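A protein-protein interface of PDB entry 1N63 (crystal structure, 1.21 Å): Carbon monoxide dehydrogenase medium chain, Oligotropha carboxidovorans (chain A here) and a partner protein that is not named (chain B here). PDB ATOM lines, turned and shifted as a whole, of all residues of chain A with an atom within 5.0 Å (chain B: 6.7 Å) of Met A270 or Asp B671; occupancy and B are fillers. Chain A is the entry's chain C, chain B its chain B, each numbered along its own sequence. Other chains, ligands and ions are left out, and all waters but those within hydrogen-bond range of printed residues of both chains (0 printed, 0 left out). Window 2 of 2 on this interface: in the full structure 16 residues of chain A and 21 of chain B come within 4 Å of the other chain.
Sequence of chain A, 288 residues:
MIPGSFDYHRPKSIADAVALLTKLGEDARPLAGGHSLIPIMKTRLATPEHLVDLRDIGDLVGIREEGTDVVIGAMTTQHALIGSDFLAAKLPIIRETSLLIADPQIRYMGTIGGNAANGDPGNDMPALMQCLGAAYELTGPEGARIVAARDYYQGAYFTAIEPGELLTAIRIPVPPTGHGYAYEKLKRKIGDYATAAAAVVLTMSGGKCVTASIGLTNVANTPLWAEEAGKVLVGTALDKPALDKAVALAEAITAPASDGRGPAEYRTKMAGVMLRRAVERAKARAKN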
ATOM      1  N   LEU A 186      -3.846 -25.775   6.953  1.00  0.00           N
ATOM      2  CA  LEU A 186      -3.118 -25.963   5.702  1.00  0.00           C
ATOM      3  C   LEU A 186      -1.709 -25.496   5.926  1.00  0.00           C
ATOM      4  O   LEU A 186      -1.486 -24.372   6.371  1.00  0.00           O
ATOM      5  CB  LEU A 186      -3.773 -25.143   4.592  1.00  0.00           C
ATOM      6  CG  LEU A 186      -3.141 -25.129   3.212  1.00  0.00           C
ATOM      7  CD1 LEU A 186      -3.098 -26.551   2.700  1.00  0.00           C
ATOM      8  CD2 LEU A 186      -3.783 -24.172   2.235  1.00  0.00           C
ATOM      9  N   THR A 195      -0.472 -21.747   6.465  1.00  0.00           N
ATOM     10  CA  THR A 195      -0.938 -20.918   5.381  1.00  0.00           C
ATOM     11  C   THR A 195      -2.278 -20.266   5.741  1.00  0.00           C
ATOM     12  O   THR A 195      -2.472 -19.076   5.567  1.00  0.00           O
ATOM     13  CB  THR A 195      -1.034 -21.785   4.131  1.00  0.00           C
ATOM     14  OG1 THR A 195       0.262 -22.287   3.800  1.00  0.00           O
ATOM     15  CG2 THR A 195      -1.552 -21.017   2.946  1.00  0.00           C
ATOM     16  N   ALA A 196      -3.177 -21.088   6.273  1.00  0.00           N
ATOM     17  CA  ALA A 196      -4.417 -20.657   6.923  1.00  0.00           C
ATOM     18  C   ALA A 196      -4.865 -21.843   7.775  1.00  0.00           C
ATOM     19  O   ALA A 196      -4.577 -22.996   7.456  1.00  0.00           O
ATOM     20  CB  ALA A 196      -5.439 -20.326   5.904  1.00  0.00           C
ATOM     21  N   TYR A 266      -4.425 -15.726  -1.974  1.00  0.00           N
ATOM     22  CA  TYR A 266      -4.444 -17.165  -1.797  1.00  0.00           C
ATOM     23  C   TYR A 266      -4.732 -17.538  -0.343  1.00  0.00           C
ATOM     24  O   TYR A 266      -5.614 -18.373  -0.046  1.00  0.00           O
ATOM     25  CB  TYR A 266      -3.137 -17.826  -2.266  1.00  0.00           C
ATOM     26  CG  TYR A 266      -3.025 -19.274  -1.861  1.00  0.00           C
ATOM     27  CD1 TYR A 266      -3.894 -20.210  -2.389  1.00  0.00           C
ATOM     28  CD2 TYR A 266      -2.036 -19.723  -1.000  1.00  0.00           C
ATOM     29  CE1 TYR A 266      -3.711 -21.592  -2.168  1.00  0.00           C
ATOM     30  CE2 TYR A 266      -1.865 -21.078  -0.780  1.00  0.00           C
ATOM     31  CZ  TYR A 266      -2.740 -21.996  -1.297  1.00  0.00           C
ATOM     32  OH  TYR A 266      -2.622 -23.344  -1.051  1.00  0.00           O
ATOM     33  N   ARG A 267      -4.067 -16.856   0.573  1.00  0.00           N
ATOM     34  CA  ARG A 267      -4.265 -17.161   1.969  1.00  0.00           C
ATOM     35  C   ARG A 267      -5.668 -16.819   2.485  1.00  0.00           C
ATOM     36  O   ARG A 267      -6.249 -17.580   3.236  1.00  0.00           O
ATOM     37  CB  ARG A 267      -3.170 -16.580   2.812  1.00  0.00           C
ATOM     38  CG  ARG A 267      -1.818 -17.111   2.380  1.00  0.00           C
ATOM     39  CD  ARG A 267      -0.700 -16.517   3.154  1.00  0.00           C
ATOM     40  NE  ARG A 267      -0.706 -17.002   4.538  1.00  0.00           N
ATOM     41  CZ  ARG A 267       0.270 -16.748   5.363  1.00  0.00           C
ATOM     42  NH1 ARG A 267       1.174 -15.863   5.019  1.00  0.00           N
ATOM     43  NH2 ARG A 267       0.343 -17.344   6.545  1.00  0.00           N
ATOM     44  N   THR A 268      -6.246 -15.741   1.980  1.00  0.00           N
ATOM     45  CA  THR A 268      -7.628 -15.406   2.312  1.00  0.00           C
ATOM     46  C   THR A 268      -8.560 -16.498   1.782  1.00  0.00           C
ATOM     47  O   THR A 268      -9.431 -16.968   2.502  1.00  0.00           O
ATOM     48  CB  THR A 268      -7.947 -14.060   1.658  1.00  0.00           C
ATOM     49  OG1 THR A 268      -7.260 -13.020   2.384  1.00  0.00           O
ATOM     50  CG2 THR A 268      -9.438 -13.763   1.731  1.00  0.00           C
ATOM     51  N   LYS A 269      -8.312 -16.954   0.557  1.00  0.00           N
ATOM     52  CA  LYS A 269      -9.161 -18.014   0.028  1.00  0.00           C
ATOM     53  C   LYS A 269      -8.993 -19.298   0.824  1.00  0.00           C
ATOM     54  O   LYS A 269      -9.967 -20.019   1.032  1.00  0.00           O
ATOM     55  CB  LYS A 269      -8.944 -18.211  -1.469  1.00  0.00           C
ATOM     56  CG  LYS A 269      -9.296 -17.007  -2.305  1.00  0.00           C
ATOM     57  CD  LYS A 269     -10.822 -16.794  -2.247  1.00  0.00           C
ATOM     58  CE  LYS A 269     -11.360 -15.604  -3.028  1.00  0.00           C
ATOM     59  NZ  LYS A 269     -12.808 -15.454  -2.710  1.00  0.00           N
ATOM     60  N   MET A 270      -7.779 -19.590   1.265  1.00  0.00           N
ATOM     61  CA  MET A 270      -7.580 -20.801   2.039  1.00  0.00           C
ATOM     62  C   MET A 270      -8.227 -20.694   3.392  1.00  0.00           C
ATOM     63  O   MET A 270      -8.603 -21.739   3.922  1.00  0.00           O
ATOM     64  CB  MET A 270      -6.097 -21.143   2.132  1.00  0.00           C
ATOM     65  CG  MET A 270      -5.432 -21.440   0.770  1.00  0.00           C
ATOM     66  SD  MET A 270      -6.309 -22.849  -0.092  1.00  0.00           S
ATOM     67  CE  MET A 270      -7.328 -21.943  -1.250  1.00  0.00           C
ATOM     68  N   ALA A 271      -8.296 -19.511   3.980  1.00  0.00           N
ATOM     69  CA  ALA A 271      -9.045 -19.377   5.218  1.00  0.00           C
ATOM     70  C   ALA A 271     -10.483 -19.882   5.003  1.00  0.00           C
ATOM     71  O   ALA A 271     -11.071 -20.560   5.844  1.00  0.00           O
ATOM     72  CB  ALA A 271      -9.013 -17.989   5.728  1.00  0.00           C
ATOM     73  N   GLY A 272     -11.082 -19.492   3.886  1.00  0.00           N
ATOM     74  CA  GLY A 272     -12.417 -19.964   3.561  1.00  0.00           C
ATOM     75  C   GLY A 272     -12.516 -21.449   3.331  1.00  0.00           C
ATOM     76  O   GLY A 272     -13.481 -22.077   3.791  1.00  0.00           O
ATOM     77  N   VAL A 273     -11.530 -22.035   2.626  1.00  0.00           N
ATOM     78  CA  VAL A 273     -11.590 -23.466   2.428  1.00  0.00           C
ATOM     79  C   VAL A 273     -11.441 -24.211   3.739  1.00  0.00           C
ATOM     80  O   VAL A 273     -12.157 -25.213   4.006  1.00  0.00           O
ATOM     81  CB  VAL A 273     -10.499 -23.905   1.391  1.00  0.00           C
ATOM     82  CG1 VAL A 273     -10.526 -25.445   1.233  1.00  0.00           C
ATOM     83  CG2 VAL A 273     -10.735 -23.223   0.033  1.00  0.00           C
ATOM     84  N   MET A 274     -10.476 -23.789   4.548  1.00  0.00           N
ATOM     85  CA  MET A 274     -10.300 -24.393   5.857  1.00  0.00           C
ATOM     86  C   MET A 274     -11.560 -24.283   6.700  1.00  0.00           C
ATOM     87  O   MET A 274     -11.898 -25.203   7.422  1.00  0.00           O
ATOM     88  CB  MET A 274      -9.069 -23.840   6.585  1.00  0.00           C
ATOM     89  CG  MET A 274      -7.710 -24.135   5.913  1.00  0.00           C
ATOM     90  SD  MET A 274      -7.405 -25.877   5.658  1.00  0.00           S
ATOM     91  CE  MET A 274      -7.681 -26.018   3.952  1.00  0.00           C
ATOM     92  N   LEU A 275     -12.229 -23.136   6.674  1.00  0.00           N
ATOM     93  CA  LEU A 275     -13.467 -22.967   7.384  1.00  0.00           C
ATOM     94  C   LEU A 275     -14.528 -23.971   6.930  1.00  0.00           C
ATOM     95  O   LEU A 275     -15.124 -24.683   7.743  1.00  0.00           O
ATOM     96  CB  LEU A 275     -13.941 -21.503   7.257  1.00  0.00           C
ATOM     97  CG  LEU A 275     -15.303 -21.255   7.868  1.00  0.00           C
ATOM     98  CD1 LEU A 275     -15.290 -21.781   9.301  1.00  0.00           C
ATOM     99  CD2 LEU A 275     -15.657 -19.792   7.767  1.00  0.00           C
ATOM    100  N   ARG B 476     -13.228 -32.491  -7.359  1.00  0.00           N
ATOM    101  CA  ARG B 476     -12.322 -31.368  -7.557  1.00  0.00           C
ATOM    102  C   ARG B 476     -10.878 -31.846  -7.531  1.00  0.00           C
ATOM    103  O   ARG B 476      -9.968 -31.038  -7.535  1.00  0.00           O
ATOM    104  CB  ARG B 476     -12.542 -30.377  -6.420  1.00  0.00           C
ATOM    105  CG  ARG B 476     -13.978 -29.817  -6.357  1.00  0.00           C
ATOM    106  CD  ARG B 476     -14.375 -29.084  -7.630  1.00  0.00           C
ATOM    107  NE  ARG B 476     -13.545 -27.907  -7.807  1.00  0.00           N
ATOM    108  CZ  ARG B 476     -13.477 -27.169  -8.911  1.00  0.00           C
ATOM    109  NH1 ARG B 476     -14.117 -27.495 -10.020  1.00  0.00           N
ATOM    110  NH2 ARG B 476     -12.857 -26.009  -8.865  1.00  0.00           N
ATOM    111  N   ILE B 668      -4.282 -34.179  -7.432  1.00  0.00           N
ATOM    112  CA  ILE B 668      -4.193 -32.780  -7.087  1.00  0.00           C
ATOM    113  C   ILE B 668      -5.592 -32.216  -6.822  1.00  0.00           C
ATOM    114  O   ILE B 668      -6.530 -32.394  -7.627  1.00  0.00           O
ATOM    115  CB  ILE B 668      -3.527 -31.988  -8.186  1.00  0.00           C
ATOM    116  CG1 ILE B 668      -2.223 -32.686  -8.640  1.00  0.00           C
ATOM    117  CG2 ILE B 668      -3.353 -30.534  -7.751  1.00  0.00           C
ATOM    118  CD1 ILE B 668      -1.507 -31.972  -9.757  1.00  0.00           C
ATOM    119  N   ASP B 669      -5.745 -31.517  -5.707  1.00  0.00           N
ATOM    120  CA  ASP B 669      -6.953 -30.771  -5.336  1.00  0.00           C
ATOM    121  C   ASP B 669      -6.829 -29.420  -5.963  1.00  0.00           C
ATOM    122  O   ASP B 669      -5.962 -28.614  -5.560  1.00  0.00           O
ATOM    123  CB  ASP B 669      -7.007 -30.638  -3.810  1.00  0.00           C
ATOM    124  CG  ASP B 669      -8.209 -29.926  -3.286  1.00  0.00           C
ATOM    125  OD1 ASP B 669      -8.700 -28.941  -3.889  1.00  0.00           O
ATOM    126  OD2 ASP B 669      -8.624 -30.283  -2.173  1.00  0.00           O
ATOM    127  N   VAL B 670      -7.672 -29.146  -6.964  1.00  0.00           N
ATOM    128  CA  VAL B 670      -7.564 -27.909  -7.710  1.00  0.00           C
ATOM    129  C   VAL B 670      -7.938 -26.664  -6.937  1.00  0.00           C
ATOM    130  O   VAL B 670      -7.540 -25.560  -7.300  1.00  0.00           O
ATOM    131  CB  VAL B 670      -8.286 -27.940  -9.085  1.00  0.00           C
ATOM    132  CG1 VAL B 670      -7.900 -29.139  -9.895  1.00  0.00           C
ATOM    133  CG2 VAL B 670      -9.797 -27.949  -8.889  1.00  0.00           C
ATOM    134  N   ASP B 671      -8.715 -26.820  -5.863  1.00  0.00           N
ATOM    135  CA  ASP B 671      -9.174 -25.694  -5.033  1.00  0.00           C
ATOM    136  C   ASP B 671      -8.162 -25.277  -3.982  1.00  0.00           C
ATOM    137  O   ASP B 671      -8.176 -24.086  -3.672  1.00  0.00           O
ATOM    138  CB  ASP B 671     -10.495 -26.074  -4.403  1.00  0.00           C
ATOM    139  CG  ASP B 671     -11.592 -26.129  -5.433  1.00  0.00           C
ATOM    140  OD1 ASP B 671     -11.511 -25.405  -6.468  1.00  0.00           O
ATOM    141  OD2 ASP B 671     -12.534 -26.936  -5.332  1.00  0.00           O
ATOM    142  N   THR B 672      -7.243 -26.147  -3.550  1.00  0.00           N
ATOM    143  CA  THR B 672      -6.192 -25.690  -2.613  1.00  0.00           C
ATOM    144  C   THR B 672      -4.825 -25.677  -3.317  1.00  0.00           C
ATOM    145  O   THR B 672      -3.870 -25.144  -2.744  1.00  0.00           O
ATOM    146  CB  THR B 672      -6.096 -26.588  -1.404  1.00  0.00           C
ATOM    147  OG1 THR B 672      -5.829 -27.917  -1.875  1.00  0.00           O
ATOM    148  CG2 THR B 672      -7.421 -26.606  -0.639  1.00  0.00           C
ATOM    149  N   GLY B 673      -4.654 -26.443  -4.410  1.00  0.00           N
ATOM    150  CA  GLY B 673      -3.344 -26.666  -5.044  1.00  0.00           C
ATOM    151  C   GLY B 673      -2.545 -27.735  -4.391  1.00  0.00           C
ATOM    152  O   GLY B 673      -1.428 -27.989  -4.850  1.00  0.00           O
ATOM    153  N   VAL B 674      -3.119 -28.487  -3.438  1.00  0.00           N
ATOM    154  CA  VAL B 674      -2.372 -29.547  -2.746  1.00  0.00           C
ATOM    155  C   VAL B 674      -2.295 -30.827  -3.567  1.00  0.00           C
ATOM    156  O   VAL B 674      -3.308 -31.354  -3.995  1.00  0.00           O
ATOM    157  CB  VAL B 674      -2.968 -29.849  -1.359  1.00  0.00           C
ATOM    158  CG1 VAL B 674      -2.252 -31.035  -0.728  1.00  0.00           C
ATOM    159  CG2 VAL B 674      -2.877 -28.624  -0.432  1.00  0.00           C
ATOM    160  N   TYR B 781      -2.966 -31.378 -15.360  1.00  0.00           N
ATOM    161  CA  TYR B 781      -3.634 -30.190 -15.844  1.00  0.00           C
ATOM    162  C   TYR B 781      -3.777 -30.151 -17.359  1.00  0.00           C
ATOM    163  O   TYR B 781      -4.356 -29.186 -17.863  1.00  0.00           O
ATOM    164  CB  TYR B 781      -2.911 -28.931 -15.374  1.00  0.00           C
ATOM    165  CG  TYR B 781      -3.183 -28.586 -13.919  1.00  0.00           C
ATOM    166  CD1 TYR B 781      -4.299 -27.846 -13.541  1.00  0.00           C
ATOM    167  CD2 TYR B 781      -2.356 -28.994 -12.908  1.00  0.00           C
ATOM    168  CE1 TYR B 781      -4.533 -27.480 -12.221  1.00  0.00           C
ATOM    169  CE2 TYR B 781      -2.563 -28.613 -11.603  1.00  0.00           C
ATOM    170  CZ  TYR B 781      -3.663 -27.938 -11.226  1.00  0.00           C
ATOM    171  OH  TYR B 781      -3.877 -27.620  -9.895  1.00  0.00           O
ATOM    172  N   TRP B 799      -2.557 -23.587  -7.031  1.00  0.00           N
ATOM    173  CA  TRP B 799      -3.791 -22.795  -6.866  1.00  0.00           C
ATOM    174  C   TRP B 799      -3.845 -21.712  -7.948  1.00  0.00           C
ATOM    175  O   TRP B 799      -4.858 -21.514  -8.587  1.00  0.00           O
ATOM    176  CB  TRP B 799      -3.927 -22.215  -5.461  1.00  0.00           C
ATOM    177  CG  TRP B 799      -5.043 -21.250  -5.326  1.00  0.00           C
ATOM    178  CD1 TRP B 799      -6.345 -21.522  -4.988  1.00  0.00           C
ATOM    179  CD2 TRP B 799      -4.973 -19.848  -5.580  1.00  0.00           C
ATOM    180  NE1 TRP B 799      -7.048 -20.344  -4.936  1.00  0.00           N
ATOM    181  CE2 TRP B 799      -6.223 -19.302  -5.291  1.00  0.00           C
ATOM    182  CE3 TRP B 799      -3.948 -18.985  -5.998  1.00  0.00           C
ATOM    183  CZ2 TRP B 799      -6.499 -17.955  -5.510  1.00  0.00           C
ATOM    184  CZ3 TRP B 799      -4.170 -17.638  -6.027  1.00  0.00           C
ATOM    185  CH2 TRP B 799      -5.441 -17.133  -5.812  1.00  0.00           C
ATOM    186  N   LEU B 807     -10.941 -21.987 -12.782  1.00  0.00           N
ATOM    187  CA  LEU B 807     -11.472 -23.104 -11.983  1.00  0.00           C
ATOM    188  C   LEU B 807     -12.127 -22.711 -10.669  1.00  0.00           C
ATOM    189  O   LEU B 807     -12.822 -23.529 -10.062  1.00  0.00           O
ATOM    190  CB  LEU B 807     -10.364 -24.113 -11.693  1.00  0.00           C
ATOM    191  CG  LEU B 807      -9.600 -24.680 -12.892  1.00  0.00           C
ATOM    192  CD1 LEU B 807      -8.679 -25.811 -12.517  1.00  0.00           C
ATOM    193  CD2 LEU B 807     -10.571 -25.184 -13.944  1.00  0.00           C
ATOM    194  N   HIS B 808     -11.846 -21.523 -10.165  1.00  0.00           N
ATOM    195  CA  HIS B 808     -12.418 -21.125  -8.875  1.00  0.00           C
ATOM    196  C   HIS B 808     -13.604 -20.185  -8.945  1.00  0.00           C
ATOM    197  O   HIS B 808     -14.080 -19.698  -7.896  1.00  0.00           O
ATOM    198  CB  HIS B 808     -11.356 -20.514  -7.979  1.00  0.00           C
ATOM    199  CG  HIS B 808     -10.076 -21.307  -7.889  1.00  0.00           C
ATOM    200  ND1 HIS B 808      -9.990 -22.676  -7.679  1.00  0.00           N
ATOM    201  CD2 HIS B 808      -8.809 -20.848  -7.877  1.00  0.00           C
ATOM    202  CE1 HIS B 808      -8.708 -23.018  -7.613  1.00  0.00           C
ATOM    203  NE2 HIS B 808      -7.972 -21.927  -7.758  1.00  0.00           N
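The guanidinium group of Arg B476 lies within salt-bridge range of the side-chain carboxylate of Asp B671, 2.8 Å away. OD1 of Asp B669 is in hydrogen-bond range of N of Asp B671 (2.9 Å). OD1 of Asp B669 is in hydrogen-bond range of N of Thr B672 (3.2 Å). N of Asp B669 sits at hydrogen-bond distance from O of Val B674, 3.0 Å away. The side-chain carboxylate (OD1) of Asp B671 sits at hydrogen-bond distance from a ring nitrogen (ND1) of His B808 (3.4 Å). O of Ala A196 sits at hydrogen-bond distance from N of Leu A186, at 2.9 Å.
Of chain B, only Asp B671, Thr B672 and Trp B799 come within 4 Å of Met A270. Asp B671 touches just one residue of chain A: Met A270. Of the printed residues of chain A, Trp B799 touches Tyr A266 and Met A270. Of the printed residues of chain B, Val A273 touches Thr B672. Printed residues of chain B within 4 Å of Leu A186: Val B674 (3.8 Å). Asp B669 touches none of the printed residues of chain A. Ala A196 touches none of the printed residues of chain B. The nearest residue of chain A that does not touch Asp B671 is Val A273 (4.6 Å). The nearest printed residue of chain B that does not touch Tyr A266 is Gly B673 (5.0 Å).
Hydrophobic or aromatic side chains of chain B within 4 Å of the printed part of chain A: Val B674 and Trp B799. Along chain B the printed residues that touch a printed residue of chain A span positions 671 to 799. Of the 13 printed residues of chain A, 4 touch a printed residue of chain B. Along chain A the printed residues that touch a printed residue of chain B span positions 186 to 273. Among the printed residues, 7 pairs touch across the chains. Among the printed residues, no Asp or Glu carboxylate lies within 4 Å of a Lys or Arg side-chain nitrogen of the other chain.
CD1 of Leu A186 touches CG2 of Val B674, 3.8 Å away. Tyr A266 touches Trp B799 (CD1 to CG, 3.3 Å). Met A270 touches Asp B671 (CE to O, 3.3 Å). Thr B672 touches Met A270. CD1 of Trp B799 touches CE of Met A270, 3.9 Å away. CG1 of Val A273 touches CG2 of Thr B672, at 3.8 Å.
O of Thr B672 sits at hydrogen-bond distance from OH of Tyr A266 (2.8 Å).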
